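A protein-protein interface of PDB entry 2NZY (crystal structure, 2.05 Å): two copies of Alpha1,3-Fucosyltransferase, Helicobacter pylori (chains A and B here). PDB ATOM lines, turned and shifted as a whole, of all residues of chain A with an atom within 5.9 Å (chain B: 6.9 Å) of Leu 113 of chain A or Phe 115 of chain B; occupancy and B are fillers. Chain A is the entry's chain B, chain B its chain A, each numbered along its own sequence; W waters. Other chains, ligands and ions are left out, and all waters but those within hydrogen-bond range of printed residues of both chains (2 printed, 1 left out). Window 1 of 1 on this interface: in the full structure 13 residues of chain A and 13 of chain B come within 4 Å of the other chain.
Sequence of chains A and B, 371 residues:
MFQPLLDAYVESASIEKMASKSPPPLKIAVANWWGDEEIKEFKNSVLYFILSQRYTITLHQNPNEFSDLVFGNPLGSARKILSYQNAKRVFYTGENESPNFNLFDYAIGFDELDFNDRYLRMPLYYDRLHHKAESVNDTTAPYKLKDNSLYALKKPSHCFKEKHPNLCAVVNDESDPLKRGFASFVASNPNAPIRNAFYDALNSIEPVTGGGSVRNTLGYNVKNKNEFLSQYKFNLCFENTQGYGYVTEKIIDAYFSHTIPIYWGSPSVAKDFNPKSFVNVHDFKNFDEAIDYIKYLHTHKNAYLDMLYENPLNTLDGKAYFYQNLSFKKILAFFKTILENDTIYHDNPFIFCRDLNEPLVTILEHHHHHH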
ATOM      1  N   SER A  98      15.988  29.639 -10.784  1.00  0.00           N
ATOM      2  CA  SER A  98      17.343  29.267 -10.317  1.00  0.00           C
ATOM      3  C   SER A  98      18.312  29.483 -11.502  1.00  0.00           C
ATOM      4  O   SER A  98      17.926  29.357 -12.672  1.00  0.00           O
ATOM      5  CB  SER A  98      17.355  27.824  -9.832  1.00  0.00           C
ATOM      6  OG  SER A  98      16.516  27.709  -8.714  1.00  0.00           O
ATOM      7  N   PRO A  99      19.557  29.858 -11.219  1.00  0.00           N
ATOM      8  CA  PRO A  99      20.516  30.108 -12.301  1.00  0.00           C
ATOM      9  C   PRO A  99      20.955  28.887 -13.068  1.00  0.00           C
ATOM     10  O   PRO A  99      20.971  27.787 -12.526  1.00  0.00           O
ATOM     11  CB  PRO A  99      21.740  30.687 -11.574  1.00  0.00           C
ATOM     12  CG  PRO A  99      21.286  30.968 -10.189  1.00  0.00           C
ATOM     13  CD  PRO A  99      20.202  30.009  -9.908  1.00  0.00           C
ATOM     14  N   PHE A 101      24.167  27.513 -14.376  1.00  0.00           N
ATOM     15  CA  PHE A 101      25.602  27.675 -14.205  1.00  0.00           C
ATOM     16  C   PHE A 101      26.415  27.114 -15.352  1.00  0.00           C
ATOM     17  O   PHE A 101      27.655  27.233 -15.350  1.00  0.00           O
ATOM     18  CB  PHE A 101      26.046  27.037 -12.850  1.00  0.00           C
ATOM     19  CG  PHE A 101      25.552  27.807 -11.654  1.00  0.00           C
ATOM     20  CD1 PHE A 101      26.094  29.071 -11.349  1.00  0.00           C
ATOM     21  CD2 PHE A 101      24.533  27.314 -10.853  1.00  0.00           C
ATOM     22  CE1 PHE A 101      25.632  29.819 -10.260  1.00  0.00           C
ATOM     23  CE2 PHE A 101      24.068  28.088  -9.728  1.00  0.00           C
ATOM     24  CZ  PHE A 101      24.629  29.330  -9.449  1.00  0.00           C
ATOM     25  N   PHE A 110      17.825  34.454  -5.630  1.00  0.00           N
ATOM     26  CA  PHE A 110      17.069  34.234  -4.423  1.00  0.00           C
ATOM     27  C   PHE A 110      17.396  32.920  -3.724  1.00  0.00           C
ATOM     28  O   PHE A 110      17.143  32.773  -2.541  1.00  0.00           O
ATOM     29  CB  PHE A 110      15.533  34.124  -4.714  1.00  0.00           C
ATOM     30  CG  PHE A 110      14.898  35.390  -5.283  1.00  0.00           C
ATOM     31  CD1 PHE A 110      14.784  35.563  -6.667  1.00  0.00           C
ATOM     32  CD2 PHE A 110      14.372  36.396  -4.426  1.00  0.00           C
ATOM     33  CE1 PHE A 110      14.148  36.731  -7.208  1.00  0.00           C
ATOM     34  CE2 PHE A 110      13.715  37.593  -4.957  1.00  0.00           C
ATOM     35  CZ  PHE A 110      13.617  37.736  -6.364  1.00  0.00           C
ATOM     36  N   ASP A 111      17.857  31.929  -4.470  1.00  0.00           N
ATOM     37  CA  ASP A 111      18.084  30.652  -3.866  1.00  0.00           C
ATOM     38  C   ASP A 111      18.925  30.633  -2.626  1.00  0.00           C
ATOM     39  O   ASP A 111      19.858  31.432  -2.457  1.00  0.00           O
ATOM     40  CB  ASP A 111      18.670  29.707  -4.911  1.00  0.00           C
ATOM     41  CG  ASP A 111      17.608  29.306  -5.943  1.00  0.00           C
ATOM     42  OD1 ASP A 111      16.558  28.722  -5.534  1.00  0.00           O
ATOM     43  OD2 ASP A 111      17.827  29.575  -7.141  1.00  0.00           O
ATOM     44  N   GLU A 112      18.582  29.695  -1.753  1.00  0.00           N
ATOM     45  CA  GLU A 112      19.345  29.498  -0.540  1.00  0.00           C
ATOM     46  C   GLU A 112      20.412  28.463  -0.919  1.00  0.00           C
ATOM     47  O   GLU A 112      20.282  27.271  -0.592  1.00  0.00           O
ATOM     48  CB  GLU A 112      18.452  28.926   0.512  1.00  0.00           C
ATOM     49  CG  GLU A 112      17.413  29.936   1.027  1.00  0.00           C
ATOM     50  CD  GLU A 112      16.642  29.345   2.190  1.00  0.00           C
ATOM     51  OE1 GLU A 112      17.203  29.286   3.306  1.00  0.00           O
ATOM     52  OE2 GLU A 112      15.506  28.882   1.977  1.00  0.00           O
ATOM     53  N   LEU A 113      21.447  28.907  -1.599  1.00  0.00           N
ATOM     54  CA  LEU A 113      22.475  27.990  -2.044  1.00  0.00           C
ATOM     55  C   LEU A 113      23.893  28.581  -1.936  1.00  0.00           C
ATOM     56  O   LEU A 113      24.077  29.790  -1.985  1.00  0.00           O
ATOM     57  CB  LEU A 113      22.168  27.520  -3.466  1.00  0.00           C
ATOM     58  CG  LEU A 113      22.714  28.119  -4.741  1.00  0.00           C
ATOM     59  CD1 LEU A 113      24.168  27.707  -4.880  1.00  0.00           C
ATOM     60  CD2 LEU A 113      21.905  27.610  -5.939  1.00  0.00           C
ATOM     61  N   ASP A 114      24.868  27.700  -1.783  1.00  0.00           N
ATOM     62  CA  ASP A 114      26.246  28.118  -1.639  1.00  0.00           C
ATOM     63  C   ASP A 114      27.088  27.487  -2.713  1.00  0.00           C
ATOM     64  O   ASP A 114      27.215  26.257  -2.822  1.00  0.00           O
ATOM     65  CB  ASP A 114      26.703  27.757  -0.233  1.00  0.00           C
ATOM     66  CG  ASP A 114      28.173  28.067   0.028  1.00  0.00           C
ATOM     67  OD1 ASP A 114      28.847  28.723  -0.790  1.00  0.00           O
ATOM     68  OD2 ASP A 114      28.660  27.624   1.094  1.00  0.00           O
ATOM     69  N   PHE A 115      27.603  28.341  -3.589  1.00  0.00           N
ATOM     70  CA  PHE A 115      28.431  27.837  -4.662  1.00  0.00           C
ATOM     71  C   PHE A 115      29.748  28.637  -4.629  1.00  0.00           C
ATOM     72  O   PHE A 115      30.265  29.036  -5.678  1.00  0.00           O
ATOM     73  CB  PHE A 115      27.697  28.025  -6.015  1.00  0.00           C
ATOM     74  CG  PHE A 115      28.152  27.085  -7.096  1.00  0.00           C
ATOM     75  CD1 PHE A 115      29.220  26.211  -6.878  1.00  0.00           C
ATOM     76  CD2 PHE A 115      27.558  27.120  -8.375  1.00  0.00           C
ATOM     77  CE1 PHE A 115      29.707  25.375  -7.931  1.00  0.00           C
ATOM     78  CE2 PHE A 115      28.023  26.299  -9.431  1.00  0.00           C
ATOM     79  CZ  PHE A 115      29.097  25.429  -9.220  1.00  0.00           C
ATOM     80  N   TYR A 119      28.080  32.321  -6.683  1.00  0.00           N
ATOM     81  CA  TYR A 119      26.707  32.736  -6.405  1.00  0.00           C
ATOM     82  C   TYR A 119      26.518  33.692  -5.220  1.00  0.00           C
ATOM     83  O   TYR A 119      27.114  33.544  -4.193  1.00  0.00           O
ATOM     84  CB  TYR A 119      25.872  31.497  -6.184  1.00  0.00           C
ATOM     85  CG  TYR A 119      24.435  31.768  -5.847  1.00  0.00           C
ATOM     86  CD1 TYR A 119      23.518  32.105  -6.841  1.00  0.00           C
ATOM     87  CD2 TYR A 119      24.006  31.776  -4.520  1.00  0.00           C
ATOM     88  CE1 TYR A 119      22.198  32.462  -6.520  1.00  0.00           C
ATOM     89  CE2 TYR A 119      22.685  32.139  -4.181  1.00  0.00           C
ATOM     90  CZ  TYR A 119      21.794  32.486  -5.187  1.00  0.00           C
ATOM     91  OH  TYR A 119      20.500  32.889  -4.849  1.00  0.00           O
ATOM     92  N   ARG A 121      23.264  35.535  -3.000  1.00  0.00           N
ATOM     93  CA  ARG A 121      21.851  35.701  -2.770  1.00  0.00           C
ATOM     94  C   ARG A 121      21.595  37.200  -2.536  1.00  0.00           C
ATOM     95  O   ARG A 121      22.144  37.777  -1.589  1.00  0.00           O
ATOM     96  CB  ARG A 121      21.358  34.953  -1.519  1.00  0.00           C
ATOM     97  CG  ARG A 121      19.834  35.245  -1.258  1.00  0.00           C
ATOM     98  CD  ARG A 121      19.160  34.153  -0.404  1.00  0.00           C
ATOM     99  NE  ARG A 121      17.715  34.379  -0.271  1.00  0.00           N
ATOM    100  CZ  ARG A 121      17.124  35.048   0.711  1.00  0.00           C
ATOM    101  NH1 ARG A 121      17.839  35.612   1.743  1.00  0.00           N
ATOM    102  NH2 ARG A 121      15.792  35.144   0.652  1.00  0.00           N
ATOM    103  N   PHE B 101      18.000  23.443 -11.519  1.00  0.00           N
ATOM    104  CA  PHE B 101      17.158  23.234 -10.372  1.00  0.00           C
ATOM    105  C   PHE B 101      15.716  23.699 -10.547  1.00  0.00           C
ATOM    106  O   PHE B 101      14.898  23.514  -9.652  1.00  0.00           O
ATOM    107  CB  PHE B 101      17.781  23.824  -9.119  1.00  0.00           C
ATOM    108  CG  PHE B 101      19.011  23.062  -8.638  1.00  0.00           C
ATOM    109  CD1 PHE B 101      18.878  21.822  -7.969  1.00  0.00           C
ATOM    110  CD2 PHE B 101      20.291  23.577  -8.816  1.00  0.00           C
ATOM    111  CE1 PHE B 101      20.015  21.137  -7.488  1.00  0.00           C
ATOM    112  CE2 PHE B 101      21.430  22.882  -8.331  1.00  0.00           C
ATOM    113  CZ  PHE B 101      21.262  21.652  -7.659  1.00  0.00           C
ATOM    114  N   PHE B 104      14.422  20.053 -11.804  1.00  0.00           N
ATOM    115  CA  PHE B 104      14.687  18.913 -10.910  1.00  0.00           C
ATOM    116  C   PHE B 104      14.608  19.271  -9.456  1.00  0.00           C
ATOM    117  O   PHE B 104      15.152  20.250  -9.022  1.00  0.00           O
ATOM    118  CB  PHE B 104      16.105  18.381 -11.203  1.00  0.00           C
ATOM    119  CG  PHE B 104      16.233  17.763 -12.575  1.00  0.00           C
ATOM    120  CD1 PHE B 104      16.006  16.423 -12.746  1.00  0.00           C
ATOM    121  CD2 PHE B 104      16.472  18.550 -13.701  1.00  0.00           C
ATOM    122  CE1 PHE B 104      16.010  15.862 -14.052  1.00  0.00           C
ATOM    123  CE2 PHE B 104      16.481  18.041 -14.945  1.00  0.00           C
ATOM    124  CZ  PHE B 104      16.245  16.674 -15.139  1.00  0.00           C
ATOM    125  N   ASP B 105      13.929  18.447  -8.692  1.00  0.00           N
ATOM    126  CA  ASP B 105      13.848  18.658  -7.302  1.00  0.00           C
ATOM    127  C   ASP B 105      15.175  18.410  -6.610  1.00  0.00           C
ATOM    128  O   ASP B 105      15.540  19.126  -5.667  1.00  0.00           O
ATOM    129  CB  ASP B 105      12.796  17.720  -6.742  1.00  0.00           C
ATOM    130  CG  ASP B 105      11.438  17.970  -7.397  1.00  0.00           C
ATOM    131  OD1 ASP B 105      11.136  17.328  -8.434  1.00  0.00           O
ATOM    132  OD2 ASP B 105      10.739  18.861  -6.854  1.00  0.00           O
ATOM    133  N   LEU B 113      29.030  22.270  -4.586  1.00  0.00           N
ATOM    134  CA  LEU B 113      27.979  23.214  -4.304  1.00  0.00           C
ATOM    135  C   LEU B 113      27.174  22.649  -3.186  1.00  0.00           C
ATOM    136  O   LEU B 113      27.116  21.436  -3.009  1.00  0.00           O
ATOM    137  CB  LEU B 113      27.193  23.361  -5.587  1.00  0.00           C
ATOM    138  CG  LEU B 113      25.710  23.545  -5.816  1.00  0.00           C
ATOM    139  CD1 LEU B 113      25.644  23.418  -7.297  1.00  0.00           C
ATOM    140  CD2 LEU B 113      24.802  22.489  -5.196  1.00  0.00           C
ATOM    141  N   ASP B 114      26.584  23.537  -2.396  1.00  0.00           N
ATOM    142  CA  ASP B 114      25.804  23.095  -1.275  1.00  0.00           C
ATOM    143  C   ASP B 114      24.430  23.700  -1.444  1.00  0.00           C
ATOM    144  O   ASP B 114      24.290  24.919  -1.432  1.00  0.00           O
ATOM    145  CB  ASP B 114      26.470  23.597  -0.005  1.00  0.00           C
ATOM    146  CG  ASP B 114      25.677  23.307   1.211  1.00  0.00           C
ATOM    147  OD1 ASP B 114      24.582  22.668   1.136  1.00  0.00           O
ATOM    148  OD2 ASP B 114      26.174  23.738   2.283  1.00  0.00           O
ATOM    149  N   PHE B 115      23.420  22.856  -1.606  1.00  0.00           N
ATOM    150  CA  PHE B 115      22.015  23.321  -1.772  1.00  0.00           C
ATOM    151  C   PHE B 115      21.197  22.518  -0.754  1.00  0.00           C
ATOM    152  O   PHE B 115      20.081  22.046  -1.005  1.00  0.00           O
ATOM    153  CB  PHE B 115      21.539  23.091  -3.202  1.00  0.00           C
ATOM    154  CG  PHE B 115      20.363  23.981  -3.642  1.00  0.00           C
ATOM    155  CD1 PHE B 115      19.832  24.997  -2.803  1.00  0.00           C
ATOM    156  CD2 PHE B 115      19.821  23.827  -4.917  1.00  0.00           C
ATOM    157  CE1 PHE B 115      18.797  25.849  -3.238  1.00  0.00           C
ATOM    158  CE2 PHE B 115      18.766  24.683  -5.364  1.00  0.00           C
ATOM    159  CZ  PHE B 115      18.258  25.714  -4.510  1.00  0.00           C
ATOM    160  N   ASN B 116      21.810  22.358   0.418  1.00  0.00           N
ATOM    161  CA  ASN B 116      21.188  21.662   1.541  1.00  0.00           C
ATOM    162  C   ASN B 116      20.694  20.289   1.116  1.00  0.00           C
ATOM    163  O   ASN B 116      21.515  19.525   0.576  1.00  0.00           O
ATOM    164  CB  ASN B 116      20.102  22.550   2.133  1.00  0.00           C
ATOM    165  CG  ASN B 116      20.666  23.958   2.517  1.00  0.00           C
ATOM    166  OD1 ASN B 116      21.381  24.096   3.525  1.00  0.00           O
ATOM    167  ND2 ASN B 116      20.412  24.979   1.666  1.00  0.00           N
ATOM    168  N   ASP B 117      19.418  19.969   1.312  1.00  0.00           N
ATOM    169  CA  ASP B 117      18.916  18.644   0.969  1.00  0.00           C
ATOM    170  C   ASP B 117      18.763  18.400  -0.536  1.00  0.00           C
ATOM    171  O   ASP B 117      18.528  17.278  -0.965  1.00  0.00           O
ATOM    172  CB  ASP B 117      17.550  18.407   1.640  1.00  0.00           C
ATOM    173  CG  ASP B 117      16.457  19.475   1.180  1.00  0.00           C
ATOM    174  OD1 ASP B 117      16.824  20.681   1.002  1.00  0.00           O
ATOM    175  OD2 ASP B 117      15.243  19.117   1.014  1.00  0.00           O
ATOM    176  N   ARG B 118      18.895  19.427  -1.356  1.00  0.00           N
ATOM    177  CA  ARG B 118      18.658  19.194  -2.787  1.00  0.00           C
ATOM    178  C   ARG B 118      19.827  18.679  -3.651  1.00  0.00           C
ATOM    179  O   ARG B 118      19.627  18.350  -4.791  1.00  0.00           O
ATOM    180  CB  ARG B 118      18.095  20.495  -3.439  1.00  0.00           C
ATOM    181  CG  ARG B 118      16.715  20.984  -2.767  1.00  0.00           C
ATOM    182  CD  ARG B 118      16.029  22.197  -3.495  1.00  0.00           C
ATOM    183  NE  ARG B 118      15.687  21.817  -4.868  1.00  0.00           N
ATOM    184  CZ  ARG B 118      15.411  22.682  -5.836  1.00  0.00           C
ATOM    185  NH1 ARG B 118      15.407  23.974  -5.580  1.00  0.00           N
ATOM    186  NH2 ARG B 118      15.214  22.259  -7.077  1.00  0.00           N
ATOM    187  N   TYR B 119      21.030  18.651  -3.101  1.00  0.00           N
ATOM    188  CA  TYR B 119      22.166  18.308  -3.906  1.00  0.00           C
ATOM    189  C   TYR B 119      23.176  17.400  -3.200  1.00  0.00           C
ATOM    190  O   TYR B 119      23.467  17.601  -2.038  1.00  0.00           O
ATOM    191  CB  TYR B 119      22.910  19.609  -4.326  1.00  0.00           C
ATOM    192  CG  TYR B 119      24.152  19.310  -5.158  1.00  0.00           C
ATOM    193  CD1 TYR B 119      24.040  18.925  -6.493  1.00  0.00           C
ATOM    194  CD2 TYR B 119      25.425  19.337  -4.583  1.00  0.00           C
ATOM    195  CE1 TYR B 119      25.172  18.567  -7.265  1.00  0.00           C
ATOM    196  CE2 TYR B 119      26.558  18.981  -5.317  1.00  0.00           C
ATOM    197  CZ  TYR B 119      26.432  18.594  -6.661  1.00  0.00           C
ATOM    198  OH  TYR B 119      27.546  18.281  -7.407  1.00  0.00           O
ATOM    199  N   LEU B 120      23.708  16.430  -3.926  1.00  0.00           N
ATOM    200  CA  LEU B 120      24.756  15.503  -3.402  1.00  0.00           C
ATOM    201  C   LEU B 120      25.886  15.398  -4.445  1.00  0.00           C
ATOM    202  O   LEU B 120      25.599  15.215  -5.635  1.00  0.00           O
ATOM    203  CB  LEU B 120      24.211  14.093  -3.225  1.00  0.00           C
ATOM    204  CG  LEU B 120      25.307  13.029  -2.887  1.00  0.00           C
ATOM    205  CD1 LEU B 120      25.770  13.271  -1.424  1.00  0.00           C
ATOM    206  CD2 LEU B 120      24.769  11.575  -3.021  1.00  0.00           C
HETATM  207  O   HOH W   1      19.331  25.532 -11.686  1.00  0.00           O
HETATM  208  O   HOH W   2      14.612  25.979  -7.635  1.00  0.00           O
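The backbone NH (N) of Asp 114 of chain B is in hydrogen-bond range of the backbone carbonyl oxygen (O) of Asp 114 of chain A (2.8 Å). The backbone carbonyl oxygen of Glu 112 of chain A sits at hydrogen-bond distance from the side-chain amide nitrogen of Asn 116 of chain B, 3.2 Å away.
The backbone NH (N) of Asn 116 of chain B sits at hydrogen-bond distance from the side-chain carboxylate (OD1) of Asp 114 of chain B (2.9 Å). The side-chain hydroxyl (OG) of Ser 98 of chain A is in hydrogen-bond range of the side-chain carboxylate (OD2) of Asp 111 of chain A, 2.8 Å away. OH of Tyr 119 of chain A sits at hydrogen-bond distance from N of Asp 111 of chain A, at 2.8 Å.
OD1 of Asp 111 of chain A touches CZ of Phe 115 of chain B, 3.6 Å away. O of Glu 112 of chain A touches CD1 of Phe 115 of chain B, at 3.2 Å. Leu 113 of chain A touches Asp 114 of chain B (CA to O, 3.6 Å). Leu 113 of chain A touches Phe 115 of chain B. Leu 113 of chain B touches Asp 114 of chain A (CA to O, 3.5 Å). Phe 115 of chain A touches Leu 113 of chain B (CD1 to CB, 3.7 Å).
Of the printed residues of chain A, Asp 114 of chain B touches Leu 113 (3.6 Å) and Asp 114 (2.8 Å). Of the printed residues of chain B, Asp 114 of chain A touches Leu 113 and Asp 114. Printed residues of chain A within 4 Å of Leu 113 of chain B: Asp 114 (3.5 Å) and Phe 115 (3.7 Å). Printed residues of chain B within 4 Å of Phe 115 of chain A: Leu 113. Printed residues of chain A within 4 Å of Asn 116 of chain B: Glu 112. The nearest residue of chain B that does not touch Leu 113 of chain A is Leu 113 of chain B (4.5 Å). The nearest residue of chain A that does not touch Phe 115 of chain B is Ser 98 of chain A (5.0 Å).
Printed residues of chain A that touch a printed residue of chain B: Asp 111, Glu 112, Leu 113, Asp 114 and Phe 115. Hydrophobic or aromatic side chains of chain A that line the printed part of chain B: Leu 113 and Phe 115. Of the 11 printed residues of chain B, 4 touch a printed residue of chain A. Printed residues of chain B that touch a printed residue of chain A: Leu 113, Asp 114, Phe 115 and Asn 116. Hydrophobic or aromatic side chains of chain B within 4 Å of the printed part of chain A: Leu 113 and Phe 115. Among the printed residues, 8 pairs touch across the chains. Among the printed residues, no Asp or Glu carboxylate lies within 4 Å of a Lys or Arg side-chain nitrogen of the other chain.
Leu 113 of chain A touches Asp 114 of chain B, and with the chains exchanged Asp 114 of chain A touches Leu 113 of chain B. Leu 113 of chain A touches Phe 115 of chain B, and with the chains exchanged Phe 115 of chain A touches Leu 113 of chain B. Asp 114 of chain A touches its own counterpart, Asp 114 of chain B. 5 positions are printed for both chains.
Water W1 lies within hydrogen-bond range of N of Phe 101 of chain B and O of Pro 99 of chain A. Water W2 lies within hydrogen-bond range of the side-chain hydroxyl (OG) of Ser 98 of chain A (2.8 Å), the guanidinium group (NH1) of Arg 118 of chain B (3.0 Å) and the backbone carbonyl oxygen (O) of Phe 101 of chain B (3.2 Å).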
